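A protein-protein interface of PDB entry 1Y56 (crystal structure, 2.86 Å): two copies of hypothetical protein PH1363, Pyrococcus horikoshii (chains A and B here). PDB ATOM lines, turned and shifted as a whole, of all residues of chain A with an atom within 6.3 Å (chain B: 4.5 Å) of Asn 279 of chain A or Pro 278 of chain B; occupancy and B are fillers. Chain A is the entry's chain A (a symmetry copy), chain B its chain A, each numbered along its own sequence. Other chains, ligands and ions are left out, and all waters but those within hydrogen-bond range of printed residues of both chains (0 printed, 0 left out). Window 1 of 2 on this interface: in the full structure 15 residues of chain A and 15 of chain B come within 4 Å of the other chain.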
ATOM      1  N   THR A 256     -20.295  -0.008   2.471  1.00  0.00           N
ATOM      2  CA  THR A 256     -19.812   0.750   3.631  1.00  0.00           C
ATOM      3  C   THR A 256     -18.368   0.407   4.010  1.00  0.00           C
ATOM      4  O   THR A 256     -17.802  -0.540   3.485  1.00  0.00           O
ATOM      5  CB  THR A 256     -20.760   0.574   4.851  1.00  0.00           C
ATOM      6  OG1 THR A 256     -20.552   1.633   5.799  1.00  0.00           O
ATOM      7  CG2 THR A 256     -20.578  -0.788   5.523  1.00  0.00           C
ATOM      8  N   GLY A 257     -17.780   1.172   4.924  1.00  0.00           N
ATOM      9  CA  GLY A 257     -16.387   0.951   5.329  1.00  0.00           C
ATOM     10  C   GLY A 257     -15.423   1.924   4.666  1.00  0.00           C
ATOM     11  O   GLY A 257     -15.792   2.628   3.731  1.00  0.00           O
ATOM     12  N   ILE A 277     -23.121   4.035   2.083  1.00  0.00           N
ATOM     13  CA  ILE A 277     -23.517   4.436   3.441  1.00  0.00           C
ATOM     14  C   ILE A 277     -22.274   4.517   4.314  1.00  0.00           C
ATOM     15  O   ILE A 277     -21.809   3.493   4.818  1.00  0.00           O
ATOM     16  CB  ILE A 277     -24.513   3.421   4.121  1.00  0.00           C
ATOM     17  CG1 ILE A 277     -25.690   3.052   3.216  1.00  0.00           C
ATOM     18  CG2 ILE A 277     -25.013   3.951   5.453  1.00  0.00           C
ATOM     19  CD1 ILE A 277     -26.325   4.222   2.558  1.00  0.00           C
ATOM     20  N   PRO A 278     -21.741   5.731   4.526  1.00  0.00           N
ATOM     21  CA  PRO A 278     -20.458   5.833   5.207  1.00  0.00           C
ATOM     22  C   PRO A 278     -20.465   5.270   6.634  1.00  0.00           C
ATOM     23  O   PRO A 278     -19.422   4.830   7.123  1.00  0.00           O
ATOM     24  CB  PRO A 278     -20.190   7.341   5.220  1.00  0.00           C
ATOM     25  CG  PRO A 278     -21.531   7.954   5.114  1.00  0.00           C
ATOM     26  CD  PRO A 278     -22.273   7.056   4.182  1.00  0.00           C
ATOM     27  N   ASN A 279     -21.622   5.268   7.289  1.00  0.00           N
ATOM     28  CA  ASN A 279     -21.692   4.887   8.700  1.00  0.00           C
ATOM     29  C   ASN A 279     -22.937   4.068   9.044  1.00  0.00           C
ATOM     30  O   ASN A 279     -23.991   4.618   9.368  1.00  0.00           O
ATOM     31  CB  ASN A 279     -21.604   6.136   9.588  1.00  0.00           C
ATOM     32  CG  ASN A 279     -22.729   7.153   9.299  1.00  0.00           C
ATOM     33  OD1 ASN A 279     -23.357   7.135   8.225  1.00  0.00           O
ATOM     34  ND2 ASN A 279     -22.981   8.054  10.264  1.00  0.00           N
ATOM     35  N   VAL A 280     -22.803   2.749   8.988  1.00  0.00           N
ATOM     36  CA  VAL A 280     -23.928   1.856   9.208  1.00  0.00           C
ATOM     37  C   VAL A 280     -24.169   1.588  10.692  1.00  0.00           C
ATOM     38  O   VAL A 280     -23.237   1.233  11.432  1.00  0.00           O
ATOM     39  CB  VAL A 280     -23.720   0.538   8.463  1.00  0.00           C
ATOM     40  CG1 VAL A 280     -24.711  -0.509   8.918  1.00  0.00           C
ATOM     41  CG2 VAL A 280     -23.843   0.771   6.975  1.00  0.00           C
ATOM     42  N   LYS A 281     -25.428   1.768  11.110  1.00  0.00           N
ATOM     43  CA  LYS A 281     -25.896   1.388  12.446  1.00  0.00           C
ATOM     44  C   LYS A 281     -26.526  -0.014  12.464  1.00  0.00           C
ATOM     45  O   LYS A 281     -26.217  -0.827  13.338  1.00  0.00           O
ATOM     46  CB  LYS A 281     -26.860   2.452  13.006  1.00  0.00           C
ATOM     47  CG  LYS A 281     -27.949   1.929  13.969  1.00  0.00           C
ATOM     48  CD  LYS A 281     -28.009   2.691  15.289  1.00  0.00           C
ATOM     49  CE  LYS A 281     -28.635   4.079  15.135  1.00  0.00           C
ATOM     50  NZ  LYS A 281     -30.128   4.034  15.162  1.00  0.00           N
ATOM     51  N   ILE A 293     -29.891   0.947   8.022  1.00  0.00           N
ATOM     52  CA  ILE A 293     -30.138   2.179   8.752  1.00  0.00           C
ATOM     53  C   ILE A 293     -28.794   2.785   9.128  1.00  0.00           C
ATOM     54  O   ILE A 293     -27.934   2.075   9.640  1.00  0.00           O
ATOM     55  CB  ILE A 293     -30.943   1.910  10.054  1.00  0.00           C
ATOM     56  CG1 ILE A 293     -31.912   0.725   9.899  1.00  0.00           C
ATOM     57  CG2 ILE A 293     -31.660   3.147  10.501  1.00  0.00           C
ATOM     58  CD1 ILE A 293     -33.102   0.997   9.058  1.00  0.00           C
ATOM     59  N   ASP A 294     -28.600   4.080   8.876  1.00  0.00           N
ATOM     60  CA  ASP A 294     -27.343   4.752   9.264  1.00  0.00           C
ATOM     61  C   ASP A 294     -27.388   5.351  10.676  1.00  0.00           C
ATOM     62  O   ASP A 294     -28.392   5.234  11.375  1.00  0.00           O
ATOM     63  CB  ASP A 294     -26.853   5.764   8.197  1.00  0.00           C
ATOM     64  CG  ASP A 294     -27.773   6.977   8.030  1.00  0.00           C
ATOM     65  OD1 ASP A 294     -28.515   7.343   8.966  1.00  0.00           O
ATOM     66  OD2 ASP A 294     -27.738   7.584   6.938  1.00  0.00           O
ATOM     67  N   MET A 295     -26.297   5.987  11.091  1.00  0.00           N
ATOM     68  CA  MET A 295     -26.201   6.579  12.434  1.00  0.00           C
ATOM     69  C   MET A 295     -27.132   7.768  12.641  1.00  0.00           C
ATOM     70  O   MET A 295     -27.348   8.191  13.766  1.00  0.00           O
ATOM     71  CB  MET A 295     -24.755   6.961  12.784  1.00  0.00           C
ATOM     72  CG  MET A 295     -23.811   5.774  12.895  1.00  0.00           C
ATOM     73  SD  MET A 295     -24.314   4.581  14.161  1.00  0.00           S
ATOM     74  CE  MET A 295     -23.794   5.444  15.639  1.00  0.00           C
ATOM     75  N   ASN A 296     -27.683   8.297  11.560  1.00  0.00           N
ATOM     76  CA  ASN A 296     -28.688   9.337  11.654  1.00  0.00           C
ATOM     77  C   ASN A 296     -30.074   8.798  11.370  1.00  0.00           C
ATOM     78  O   ASN A 296     -30.971   9.558  11.017  1.00  0.00           O
ATOM     79  CB  ASN A 296     -28.370  10.472  10.682  1.00  0.00           C
ATOM     80  CG  ASN A 296     -27.082  11.184  11.025  1.00  0.00           C
ATOM     81  OD1 ASN A 296     -26.809  11.464  12.189  1.00  0.00           O
ATOM     82  ND2 ASN A 296     -26.285  11.482  10.009  1.00  0.00           N
ATOM     83  N   THR B 256     -18.400  17.761  11.374  1.00  0.00           N
ATOM     84  CA  THR B 256     -17.921  16.838  10.338  1.00  0.00           C
ATOM     85  C   THR B 256     -16.398  16.673  10.340  1.00  0.00           C
ATOM     86  O   THR B 256     -15.701  17.404  11.028  1.00  0.00           O
ATOM     87  CB  THR B 256     -18.429  17.264   8.931  1.00  0.00           C
ATOM     88  OG1 THR B 256     -18.352  16.155   8.019  1.00  0.00           O
ATOM     89  CG2 THR B 256     -17.652  18.461   8.382  1.00  0.00           C
ATOM     90  N   HIS B 276     -23.945  15.101  13.826  1.00  0.00           N
ATOM     91  CA  HIS B 276     -22.694  14.567  13.293  1.00  0.00           C
ATOM     92  C   HIS B 276     -22.918  14.117  11.836  1.00  0.00           C
ATOM     93  O   HIS B 276     -23.582  13.124  11.578  1.00  0.00           O
ATOM     94  CB  HIS B 276     -22.244  13.433  14.232  1.00  0.00           C
ATOM     95  CG  HIS B 276     -20.957  12.755  13.862  1.00  0.00           C
ATOM     96  ND1 HIS B 276     -20.073  13.250  12.925  1.00  0.00           N
ATOM     97  CD2 HIS B 276     -20.391  11.621  14.347  1.00  0.00           C
ATOM     98  CE1 HIS B 276     -19.033  12.437  12.830  1.00  0.00           C
ATOM     99  NE2 HIS B 276     -19.198  11.446  13.688  1.00  0.00           N
ATOM    100  N   ILE B 277     -22.396  14.885  10.884  1.00  0.00           N
ATOM    101  CA  ILE B 277     -22.555  14.579   9.455  1.00  0.00           C
ATOM    102  C   ILE B 277     -21.233  14.059   8.912  1.00  0.00           C
ATOM    103  O   ILE B 277     -20.349  14.852   8.581  1.00  0.00           O
ATOM    104  CB  ILE B 277     -22.965  15.834   8.594  1.00  0.00           C
ATOM    105  CG1 ILE B 277     -24.140  16.606   9.197  1.00  0.00           C
ATOM    106  CG2 ILE B 277     -23.266  15.442   7.159  1.00  0.00           C
ATOM    107  CD1 ILE B 277     -25.264  15.738   9.629  1.00  0.00           C
ATOM    108  N   PRO B 278     -21.091  12.730   8.787  1.00  0.00           N
ATOM    109  CA  PRO B 278     -19.787  12.185   8.438  1.00  0.00           C
ATOM    110  C   PRO B 278     -19.257  12.659   7.079  1.00  0.00           C
ATOM    111  O   PRO B 278     -18.042  12.712   6.881  1.00  0.00           O
ATOM    112  CB  PRO B 278     -20.033  10.673   8.429  1.00  0.00           C
ATOM    113  CG  PRO B 278     -21.482  10.538   8.175  1.00  0.00           C
ATOM    114  CD  PRO B 278     -22.095  11.668   8.933  1.00  0.00           C
ATOM    115  N   ASN B 279     -20.151  13.012   6.160  1.00  0.00           N
ATOM    116  CA  ASN B 279     -19.743  13.334   4.793  1.00  0.00           C
ATOM    117  C   ASN B 279     -20.527  14.501   4.187  1.00  0.00           C
ATOM    118  O   ASN B 279     -21.588  14.313   3.591  1.00  0.00           O
ATOM    119  CB  ASN B 279     -19.853  12.090   3.902  1.00  0.00           C
ATOM    120  CG  ASN B 279     -21.284  11.509   3.861  1.00  0.00           C
ATOM    121  OD1 ASN B 279     -22.115  11.778   4.748  1.00  0.00           O
ATOM    122  ND2 ASN B 279     -21.571  10.701   2.827  1.00  0.00           N
ATOM    123  N   VAL B 280     -19.986  15.705   4.330  1.00  0.00           N
ATOM    124  CA  VAL B 280     -20.666  16.907   3.879  1.00  0.00           C
ATOM    125  C   VAL B 280     -20.434  17.176   2.392  1.00  0.00           C
ATOM    126  O   VAL B 280     -19.285  17.175   1.921  1.00  0.00           O
ATOM    127  CB  VAL B 280     -20.228  18.114   4.706  1.00  0.00           C
ATOM    128  CG1 VAL B 280     -20.678  19.407   4.066  1.00  0.00           C
ATOM    129  CG2 VAL B 280     -20.783  17.997   6.108  1.00  0.00           C
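The backbone NH (N) of Asn 296 of chain A sits at hydrogen-bond distance from the side-chain carboxylate (OD1) of Asp 294 of chain A, 2.9 Å away. N of Met 295 of chain A is in hydrogen-bond range of O of Asn 279 of chain A, 3.2 Å away.
Among the printed residues, merely in contact across the chains: Asn 296 of chain A with His 276 of chain B, Pro 278 of chain A with Asn 279 of chain B and Asn 279 of chain A with Pro 278 of chain B.
Of the printed residues of chain B, Pro 278 of chain A touches Asn 279 (3.6 Å). Asp 294 of chain A touches none of the printed residues of chain B. Printed residues of chain B within 4 Å of Asn 296 of chain A: His 276. Of the printed residues of chain A, His 276 of chain B touches Asn 296 (3.5 Å). Ile 277 of chain B touches none of the printed residues of chain A. Of the printed residues of chain A, Pro 278 of chain B touches Asn 279. Of the printed residues of chain A, Asn 279 of chain B touches Pro 278 (3.6 Å). The nearest printed residue of chain A that does not touch Pro 278 of chain B is Pro 278 of chain A (4.01 Å).
Hydrophobic or aromatic side chains of chain B that line the printed part of chain A: Pro 278. Hydrophobic or aromatic side chains of chain A that line the printed part of chain B: Pro 278. Among the printed residues, 3 pairs touch across the chains. Among the printed residues, no Asp or Glu carboxylate lies within 4 Å of a Lys or Arg side-chain nitrogen of the other chain.
Pro 278 of chain A touches Asn 279 of chain B, and with the chains exchanged Asn 279 of chain A touches Pro 278 of chain B. 5 positions are printed for both chains.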
